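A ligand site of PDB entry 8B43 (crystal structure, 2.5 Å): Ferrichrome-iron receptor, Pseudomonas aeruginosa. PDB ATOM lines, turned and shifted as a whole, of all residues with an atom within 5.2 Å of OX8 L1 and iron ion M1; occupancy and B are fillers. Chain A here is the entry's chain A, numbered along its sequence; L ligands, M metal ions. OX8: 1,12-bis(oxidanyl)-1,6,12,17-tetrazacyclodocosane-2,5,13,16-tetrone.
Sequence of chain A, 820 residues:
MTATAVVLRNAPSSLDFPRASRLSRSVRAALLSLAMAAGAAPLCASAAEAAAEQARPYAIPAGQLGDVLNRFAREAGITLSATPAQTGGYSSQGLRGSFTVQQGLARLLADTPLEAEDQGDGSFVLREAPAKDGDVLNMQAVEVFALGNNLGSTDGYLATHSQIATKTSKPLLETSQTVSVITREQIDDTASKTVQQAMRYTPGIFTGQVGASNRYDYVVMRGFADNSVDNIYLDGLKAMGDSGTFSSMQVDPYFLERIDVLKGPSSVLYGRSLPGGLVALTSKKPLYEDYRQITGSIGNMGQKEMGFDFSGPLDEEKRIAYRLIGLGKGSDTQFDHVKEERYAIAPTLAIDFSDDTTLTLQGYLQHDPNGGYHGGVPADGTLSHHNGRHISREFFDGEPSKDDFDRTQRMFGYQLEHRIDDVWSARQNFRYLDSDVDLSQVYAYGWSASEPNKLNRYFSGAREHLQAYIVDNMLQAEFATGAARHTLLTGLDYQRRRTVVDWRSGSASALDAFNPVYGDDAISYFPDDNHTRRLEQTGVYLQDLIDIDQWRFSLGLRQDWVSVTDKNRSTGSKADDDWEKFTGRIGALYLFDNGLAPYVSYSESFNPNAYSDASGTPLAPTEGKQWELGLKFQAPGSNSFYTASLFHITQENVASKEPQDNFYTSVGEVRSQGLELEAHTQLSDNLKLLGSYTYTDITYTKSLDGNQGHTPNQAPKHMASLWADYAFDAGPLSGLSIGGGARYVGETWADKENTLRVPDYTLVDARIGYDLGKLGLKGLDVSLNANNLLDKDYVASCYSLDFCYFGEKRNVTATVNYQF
No residue comes within 4 Å of iron ion M1.
The nearest printed residue that does not touch iron ion M1 is Phe 246 (4.3 Å).
Iron ion M1 is bound by O27 of OX8 L1, O28 of OX8 L1, O23 of OX8 L1, O23 of OX8 L2, O27 of OX8 L2 and O10 of OX8 L1.
Residues that only touch OX8 L1: Val 210 (3.9 Å), Tyr 218 (3.98 Å), Phe 246 (3.6 Å), His 374 (3.2 Å), Gly 376 (3.96 Å), Gln 441 (3.0 Å), Ser 460 (3.4 Å) and Phe 803 (3.7 Å).
Ten residues have an atom within 4 Å of OX8 L1: Val 210, Tyr 218, Phe 246, His 374, Gly 376, Gln 441, Tyr 443, Ser 460, Phe 803 and Tyr 805.
The side-chain hydroxyl (OH) of Tyr 443 sits at hydrogen-bond distance from an oxygen (O19) of OX8 L1 (2.6 Å).
An oxygen (O06) of OX8 L1 lies within hydrogen-bond range of the side-chain hydroxyl (OH) of Tyr 805, 2.6 Å away.
O10 of OX8 L2 sits close to OH of Tyr 799 (2.7 Å).
The side-chain amide nitrogen of Gln 441 sits at hydrogen-bond distance from the backbone carbonyl oxygen of His 374 (3.2 Å).
O of Gln 441 lies within hydrogen-bond range of N of Ser 460 (2.8 Å).
The side-chain hydroxyl (OH) of Tyr 218 sits at hydrogen-bond distance from a ring nitrogen (NE2) of His 374, at 2.8 Å.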
ATOM      1  N   VAL A 210      -8.946 -24.231   7.706  1.00  0.00           N
ATOM      2  CA  VAL A 210     -10.249 -23.805   7.196  1.00  0.00           C
ATOM      3  C   VAL A 210     -10.134 -22.351   6.754  1.00  0.00           C
ATOM      4  O   VAL A 210     -11.093 -21.582   6.835  1.00  0.00           O
ATOM      5  CB  VAL A 210     -11.370 -23.990   8.225  1.00  0.00           C
ATOM      6  CG1 VAL A 210     -11.570 -25.458   8.528  1.00  0.00           C
ATOM      7  CG2 VAL A 210     -10.993 -23.233   9.467  1.00  0.00           C
ATOM      8  N   TYR A 218      -7.927 -23.927  14.925  1.00  0.00           N
ATOM      9  CA  TYR A 218      -7.435 -25.116  14.250  1.00  0.00           C
ATOM     10  C   TYR A 218      -5.922 -24.966  14.217  1.00  0.00           C
ATOM     11  O   TYR A 218      -5.407 -24.078  13.527  1.00  0.00           O
ATOM     12  CB  TYR A 218      -7.955 -25.178  12.819  1.00  0.00           C
ATOM     13  CG  TYR A 218      -9.402 -25.543  12.553  1.00  0.00           C
ATOM     14  CD1 TYR A 218      -9.798 -26.872  12.514  1.00  0.00           C
ATOM     15  CD2 TYR A 218     -10.375 -24.574  12.475  1.00  0.00           C
ATOM     16  CE1 TYR A 218     -11.114 -27.211  12.260  1.00  0.00           C
ATOM     17  CE2 TYR A 218     -11.702 -24.899  12.253  1.00  0.00           C
ATOM     18  CZ  TYR A 218     -12.066 -26.229  12.155  1.00  0.00           C
ATOM     19  OH  TYR A 218     -13.375 -26.572  11.912  1.00  0.00           O
ATOM     20  N   PHE A 246     -20.074 -29.599  17.982  1.00  0.00           N
ATOM     21  CA  PHE A 246     -19.806 -28.195  17.686  1.00  0.00           C
ATOM     22  C   PHE A 246     -19.307 -27.423  18.898  1.00  0.00           C
ATOM     23  O   PHE A 246     -18.956 -26.245  18.758  1.00  0.00           O
ATOM     24  CB  PHE A 246     -21.071 -27.559  17.114  1.00  0.00           C
ATOM     25  CG  PHE A 246     -21.481 -28.152  15.782  1.00  0.00           C
ATOM     26  CD1 PHE A 246     -20.746 -27.904  14.635  1.00  0.00           C
ATOM     27  CD2 PHE A 246     -22.578 -28.995  15.692  1.00  0.00           C
ATOM     28  CE1 PHE A 246     -21.102 -28.459  13.410  1.00  0.00           C
ATOM     29  CE2 PHE A 246     -22.946 -29.570  14.475  1.00  0.00           C
ATOM     30  CZ  PHE A 246     -22.202 -29.296  13.332  1.00  0.00           C
ATOM     31  N   HIS A 374     -17.990 -20.353   8.461  1.00  0.00           N
ATOM     32  CA  HIS A 374     -17.348 -21.623   8.764  1.00  0.00           C
ATOM     33  C   HIS A 374     -17.757 -22.602   7.677  1.00  0.00           C
ATOM     34  O   HIS A 374     -18.359 -23.652   7.905  1.00  0.00           O
ATOM     35  CB  HIS A 374     -17.692 -22.112  10.169  1.00  0.00           C
ATOM     36  CG  HIS A 374     -16.907 -23.325  10.589  1.00  0.00           C
ATOM     37  ND1 HIS A 374     -17.431 -24.596  10.617  1.00  0.00           N
ATOM     38  CD2 HIS A 374     -15.627 -23.440  11.029  1.00  0.00           C
ATOM     39  CE1 HIS A 374     -16.509 -25.448  11.042  1.00  0.00           C
ATOM     40  NE2 HIS A 374     -15.404 -24.773  11.291  1.00  0.00           N
ATOM     41  N   GLY A 375     -17.483 -22.244   6.418  1.00  0.00           N
ATOM     42  CA  GLY A 375     -17.895 -23.040   5.292  1.00  0.00           C
ATOM     43  C   GLY A 375     -16.717 -23.281   4.362  1.00  0.00           C
ATOM     44  O   GLY A 375     -15.592 -22.884   4.634  1.00  0.00           O
ATOM     45  N   GLY A 376     -17.014 -23.965   3.268  1.00  0.00           N
ATOM     46  CA  GLY A 376     -16.033 -24.248   2.245  1.00  0.00           C
ATOM     47  C   GLY A 376     -16.776 -24.516   0.970  1.00  0.00           C
ATOM     48  O   GLY A 376     -17.968 -24.846   0.971  1.00  0.00           O
ATOM     49  N   LEU A 439     -26.557 -23.836  16.433  1.00  0.00           N
ATOM     50  CA  LEU A 439     -26.090 -23.727  15.065  1.00  0.00           C
ATOM     51  C   LEU A 439     -27.262 -23.927  14.110  1.00  0.00           C
ATOM     52  O   LEU A 439     -28.036 -24.870  14.266  1.00  0.00           O
ATOM     53  CB  LEU A 439     -24.998 -24.745  14.779  1.00  0.00           C
ATOM     54  CG  LEU A 439     -24.637 -24.906  13.305  1.00  0.00           C
ATOM     55  CD1 LEU A 439     -23.784 -23.723  12.881  1.00  0.00           C
ATOM     56  CD2 LEU A 439     -23.908 -26.210  13.100  1.00  0.00           C
ATOM     57  N   GLN A 441     -26.925 -23.932   9.892  1.00  0.00           N
ATOM     58  CA  GLN A 441     -26.028 -23.671   8.767  1.00  0.00           C
ATOM     59  C   GLN A 441     -26.500 -24.426   7.535  1.00  0.00           C
ATOM     60  O   GLN A 441     -26.636 -25.656   7.570  1.00  0.00           O
ATOM     61  CB  GLN A 441     -24.592 -24.078   9.112  1.00  0.00           C
ATOM     62  CG  GLN A 441     -23.661 -23.955   7.923  1.00  0.00           C
ATOM     63  CD  GLN A 441     -22.251 -24.339   8.278  1.00  0.00           C
ATOM     64  OE1 GLN A 441     -21.974 -24.694   9.417  1.00  0.00           O
ATOM     65  NE2 GLN A 441     -21.373 -24.331   7.285  1.00  0.00           N
ATOM     66  N   TYR A 443     -25.022 -25.228   3.925  1.00  0.00           N
ATOM     67  CA  TYR A 443     -23.678 -25.242   3.357  1.00  0.00           C
ATOM     68  C   TYR A 443     -23.662 -25.917   2.001  1.00  0.00           C
ATOM     69  O   TYR A 443     -24.497 -26.774   1.707  1.00  0.00           O
ATOM     70  CB  TYR A 443     -22.662 -25.943   4.290  1.00  0.00           C
ATOM     71  CG  TYR A 443     -22.967 -27.387   4.585  1.00  0.00           C
ATOM     72  CD1 TYR A 443     -22.276 -28.414   3.969  1.00  0.00           C
ATOM     73  CD2 TYR A 443     -23.954 -27.731   5.501  1.00  0.00           C
ATOM     74  CE1 TYR A 443     -22.578 -29.738   4.231  1.00  0.00           C
ATOM     75  CE2 TYR A 443     -24.252 -29.044   5.782  1.00  0.00           C
ATOM     76  CZ  TYR A 443     -23.565 -30.042   5.136  1.00  0.00           C
ATOM     77  OH  TYR A 443     -23.865 -31.353   5.447  1.00  0.00           O
ATOM     78  N   TYR A 445     -22.238 -28.526  -0.671  1.00  0.00           N
ATOM     79  CA  TYR A 445     -21.578 -29.830  -0.649  1.00  0.00           C
ATOM     80  C   TYR A 445     -21.625 -30.418  -2.062  1.00  0.00           C
ATOM     81  O   TYR A 445     -22.529 -31.200  -2.384  1.00  0.00           O
ATOM     82  CB  TYR A 445     -22.285 -30.727   0.359  1.00  0.00           C
ATOM     83  CG  TYR A 445     -21.671 -32.076   0.648  1.00  0.00           C
ATOM     84  CD1 TYR A 445     -20.410 -32.416   0.153  1.00  0.00           C
ATOM     85  CD2 TYR A 445     -22.329 -32.994   1.460  1.00  0.00           C
ATOM     86  CE1 TYR A 445     -19.836 -33.659   0.442  1.00  0.00           C
ATOM     87  CE2 TYR A 445     -21.764 -34.235   1.755  1.00  0.00           C
ATOM     88  CZ  TYR A 445     -20.518 -34.566   1.238  1.00  0.00           C
ATOM     89  OH  TYR A 445     -19.943 -35.781   1.538  1.00  0.00           O
ATOM     90  N   SER A 460     -27.256 -28.325   8.330  1.00  0.00           N
ATOM     91  CA  SER A 460     -26.917 -28.903   9.613  1.00  0.00           C
ATOM     92  C   SER A 460     -27.493 -28.000  10.695  1.00  0.00           C
ATOM     93  O   SER A 460     -27.439 -26.773  10.589  1.00  0.00           O
ATOM     94  CB  SER A 460     -25.395 -29.053   9.746  1.00  0.00           C
ATOM     95  OG  SER A 460     -25.053 -29.639  10.986  1.00  0.00           O
ATOM     96  N   TYR A 799     -10.028 -29.408   2.789  1.00  0.00           N
ATOM     97  CA  TYR A 799     -10.212 -30.663   3.497  1.00  0.00           C
ATOM     98  C   TYR A 799     -10.515 -31.836   2.555  1.00  0.00           C
ATOM     99  O   TYR A 799     -10.144 -32.998   2.843  1.00  0.00           O
ATOM    100  CB  TYR A 799     -10.872 -30.323   4.834  1.00  0.00           C
ATOM    101  CG  TYR A 799     -11.345 -31.342   5.748  1.00  0.00           C
ATOM    102  CD1 TYR A 799     -10.931 -32.662   5.723  1.00  0.00           C
ATOM    103  CD2 TYR A 799     -11.431 -30.784   7.048  1.00  0.00           C
ATOM    104  CE1 TYR A 799     -11.164 -33.493   6.808  1.00  0.00           C
ATOM    105  CE2 TYR A 799     -11.554 -31.518   8.181  1.00  0.00           C
ATOM    106  CZ  TYR A 799     -11.421 -32.853   8.078  1.00  0.00           C
ATOM    107  OH  TYR A 799     -11.691 -33.536   9.223  1.00  0.00           O
ATOM    108  N   PHE A 803     -14.329 -29.499  -0.421  1.00  0.00           N
ATOM    109  CA  PHE A 803     -14.236 -28.406   0.539  1.00  0.00           C
ATOM    110  C   PHE A 803     -12.892 -27.679   0.567  1.00  0.00           C
ATOM    111  O   PHE A 803     -11.912 -28.198   1.103  1.00  0.00           O
ATOM    112  CB  PHE A 803     -14.536 -28.939   1.932  1.00  0.00           C
ATOM    113  CG  PHE A 803     -15.892 -29.550   2.053  1.00  0.00           C
ATOM    114  CD1 PHE A 803     -17.022 -28.747   2.119  1.00  0.00           C
ATOM    115  CD2 PHE A 803     -16.052 -30.925   2.050  1.00  0.00           C
ATOM    116  CE1 PHE A 803     -18.273 -29.303   2.228  1.00  0.00           C
ATOM    117  CE2 PHE A 803     -17.309 -31.485   2.152  1.00  0.00           C
ATOM    118  CZ  PHE A 803     -18.418 -30.679   2.243  1.00  0.00           C
ATOM    119  N   TYR A 805     -11.098 -23.681   1.229  1.00  0.00           N
ATOM    120  CA  TYR A 805     -11.295 -22.497   2.055  1.00  0.00           C
ATOM    121  C   TYR A 805     -10.436 -21.335   1.563  1.00  0.00           C
ATOM    122  O   TYR A 805      -9.254 -21.522   1.268  1.00  0.00           O
ATOM    123  CB  TYR A 805     -10.945 -22.853   3.487  1.00  0.00           C
ATOM    124  CG  TYR A 805     -11.572 -24.171   3.909  1.00  0.00           C
ATOM    125  CD1 TYR A 805     -12.933 -24.289   4.096  1.00  0.00           C
ATOM    126  CD2 TYR A 805     -10.782 -25.313   4.084  1.00  0.00           C
ATOM    127  CE1 TYR A 805     -13.501 -25.487   4.492  1.00  0.00           C
ATOM    128  CE2 TYR A 805     -11.341 -26.518   4.461  1.00  0.00           C
ATOM    129  CZ  TYR A 805     -12.701 -26.603   4.672  1.00  0.00           C
ATOM    130  OH  TYR A 805     -13.265 -27.815   5.013  1.00  0.00           O
HETATM  131  C13 OX8 L   1     -16.880 -31.753   6.559  1.00  0.00           C
HETATM  132  C15 OX8 L   1     -19.259 -31.960   5.626  1.00  0.00           C
HETATM  133  C20 OX8 L   1     -21.897 -31.949   9.365  1.00  0.00           C
HETATM  134  C21 OX8 L   1     -21.974 -30.473   9.761  1.00  0.00           C
HETATM  135  C22 OX8 L   1     -20.570 -29.968  10.098  1.00  0.00           C
HETATM  136  C26 OX8 L   1     -21.418 -27.663   7.935  1.00  0.00           C
HETATM  137  C01 OX8 L   1     -20.163 -28.102   7.195  1.00  0.00           C
HETATM  138  C02 OX8 L   1     -19.829 -27.073   6.116  1.00  0.00           C
HETATM  139  C03 OX8 L   1     -18.391 -27.153   5.638  1.00  0.00           C
HETATM  140  C05 OX8 L   1     -16.097 -27.014   6.482  1.00  0.00           C
HETATM  141  C07 OX8 L   1     -15.042 -26.920   7.581  1.00  0.00           C
HETATM  142  C08 OX8 L   1     -14.634 -28.328   8.021  1.00  0.00           C
HETATM  143  C09 OX8 L   1     -15.776 -28.945   8.817  1.00  0.00           C
HETATM  144  C12 OX8 L   1     -15.799 -30.939   7.282  1.00  0.00           C
HETATM  145  C14 OX8 L   1     -18.260 -31.101   6.397  1.00  0.00           C
HETATM  146  C16 OX8 L   1     -19.734 -33.239   6.332  1.00  0.00           C
HETATM  147  C18 OX8 L   1     -21.392 -32.119   7.944  1.00  0.00           C
HETATM  148  C25 OX8 L   1     -21.307 -27.668   9.471  1.00  0.00           C
HETATM  149  N04 OX8 L   1     -17.515 -27.040   6.784  1.00  0.00           N
HETATM  150  N11 OX8 L   1     -16.329 -30.235   8.449  1.00  0.00           N
HETATM  151  N17 OX8 L   1     -20.284 -33.029   7.665  1.00  0.00           N
HETATM  152  N24 OX8 L   1     -20.267 -28.548   9.940  1.00  0.00           N
HETATM  153  O06 OX8 L   1     -15.778 -27.097   5.343  1.00  0.00           O
HETATM  154  O10 OX8 L   1     -16.203 -28.351   9.750  1.00  0.00           O
HETATM  155  O19 OX8 L   1     -21.901 -31.499   7.075  1.00  0.00           O
HETATM  156  O23 OX8 L   1     -19.768 -30.738  10.477  1.00  0.00           O
HETATM  157  O27 OX8 L   1     -19.008 -27.983  10.238  1.00  0.00           O
HETATM  158  O28 OX8 L   1     -17.364 -30.791   9.199  1.00  0.00           O
HETATM  159  C13 OX8 L   2     -17.793 -34.695  11.508  1.00  0.00           C
HETATM  160  C15 OX8 L   2     -20.048 -35.155  12.449  1.00  0.00           C
HETATM  161  C20 OX8 L   2     -18.306 -32.501  14.100  1.00  0.00           C
HETATM  162  C21 OX8 L   2     -17.591 -31.192  14.457  1.00  0.00           C
HETATM  163  C22 OX8 L   2     -17.444 -30.386  13.168  1.00  0.00           C
HETATM  164  C26 OX8 L   2     -15.487 -28.078  14.733  1.00  0.00           C
HETATM  165  C01 OX8 L   2     -14.904 -29.318  15.416  1.00  0.00           C
HETATM  166  C02 OX8 L   2     -13.781 -29.977  14.635  1.00  0.00           C
HETATM  167  C03 OX8 L   2     -13.460 -29.228  13.356  1.00  0.00           C
HETATM  168  C05 OX8 L   2     -13.273 -31.306  11.951  1.00  0.00           C
HETATM  169  C07 OX8 L   2     -13.782 -32.099  10.748  1.00  0.00           C
HETATM  170  C08 OX8 L   2     -14.705 -33.242  11.136  1.00  0.00           C
HETATM  171  C09 OX8 L   2     -15.131 -33.960   9.853  1.00  0.00           C
HETATM  172  C12 OX8 L   2     -17.588 -33.661  10.411  1.00  0.00           C
HETATM  173  C14 OX8 L   2     -19.036 -35.564  11.388  1.00  0.00           C
HETATM  174  C16 OX8 L   2     -20.464 -33.709  12.203  1.00  0.00           C
HETATM  175  C18 OX8 L   2     -19.822 -32.441  14.333  1.00  0.00           C
HETATM  176  C25 OX8 L   2     -16.984 -28.238  14.443  1.00  0.00           C
HETATM  177  N04 OX8 L   2     -13.899 -30.029  12.229  1.00  0.00           N
HETATM  178  N11 OX8 L   2     -16.537 -34.132   9.533  1.00  0.00           N
HETATM  179  N17 OX8 L   2     -20.801 -33.016  13.423  1.00  0.00           N
HETATM  180  N24 OX8 L   2     -17.158 -28.960  13.187  1.00  0.00           N
HETATM  181  O06 OX8 L   2     -12.387 -31.730  12.619  1.00  0.00           O
HETATM  182  O10 OX8 L   2     -14.292 -34.363   9.112  1.00  0.00           O
HETATM  183  O19 OX8 L   2     -20.202 -31.888  15.306  1.00  0.00           O
HETATM  184  O23 OX8 L   2     -17.575 -30.926  12.131  1.00  0.00           O
HETATM  185  O27 OX8 L   2     -17.057 -28.277  11.957  1.00  0.00           O
HETATM  186  O28 OX8 L   2     -16.922 -34.783   8.350  1.00  0.00           O
HETATM  187  C13 OX8 L   3     -11.281 -38.334   6.696  1.00  0.00           C
HETATM  188  C15 OX8 L   3     -12.437 -37.859   4.521  1.00  0.00           C
HETATM  189  C20 OX8 L   3     -15.436 -34.572   3.477  1.00  0.00           C
HETATM  190  C21 OX8 L   3     -16.315 -34.517   4.714  1.00  0.00           C
HETATM  191  C22 OX8 L   3     -15.799 -35.473   5.789  1.00  0.00           C
HETATM  192  C26 OX8 L   3     -17.250 -38.161   4.044  1.00  0.00           C
HETATM  193  C01 OX8 L   3     -17.988 -39.442   4.394  1.00  0.00           C
HETATM  194  C02 OX8 L   3     -17.029 -40.525   4.886  1.00  0.00           C
HETATM  195  C03 OX8 L   3     -17.746 -41.535   5.781  1.00  0.00           C
HETATM  196  C05 OX8 L   3     -16.161 -41.316   7.676  1.00  0.00           C
HETATM  197  C07 OX8 L   3     -15.835 -40.924   9.107  1.00  0.00           C
HETATM  198  C08 OX8 L   3     -14.436 -40.326   9.060  1.00  0.00           C
HETATM  199  C09 OX8 L   3     -14.433 -38.822   8.825  1.00  0.00           C
HETATM  200  C12 OX8 L   3     -12.328 -39.121   7.482  1.00  0.00           C
HETATM  201  C14 OX8 L   3     -11.361 -38.678   5.218  1.00  0.00           C
HETATM  202  C16 OX8 L   3     -12.020 -36.394   4.350  1.00  0.00           C
HETATM  203  C18 OX8 L   3     -14.393 -35.680   3.503  1.00  0.00           C
HETATM  204  C25 OX8 L   3     -17.609 -37.025   5.005  1.00  0.00           C
HETATM  205  N04 OX8 L   3     -17.507 -41.171   7.158  1.00  0.00           N
HETATM  206  N11 OX8 L   3     -13.362 -38.244   8.014  1.00  0.00           N
HETATM  207  N17 OX8 L   3     -13.136 -35.456   4.229  1.00  0.00           N
HETATM  208  N24 OX8 L   3     -16.491 -36.751   5.901  1.00  0.00           N
HETATM  209  O06 OX8 L   3     -15.286 -41.734   6.986  1.00  0.00           O
HETATM  210  O10 OX8 L   3     -15.298 -38.154   9.288  1.00  0.00           O
HETATM  211  O19 OX8 L   3     -14.642 -36.686   2.930  1.00  0.00           O
HETATM  212  O23 OX8 L   3     -14.879 -35.167   6.488  1.00  0.00           O
HETATM  213  O27 OX8 L   3     -16.113 -37.711   6.850  1.00  0.00           O
HETATM  214  O28 OX8 L   3     -13.300 -36.865   7.758  1.00  0.00           O
HETATM  215 FE    FE M   1     -18.074 -29.605  10.555  1.00  0.00          FE
HETATM  216 FE    FE M   2     -15.673 -36.415   8.413  1.00  0.00          FE
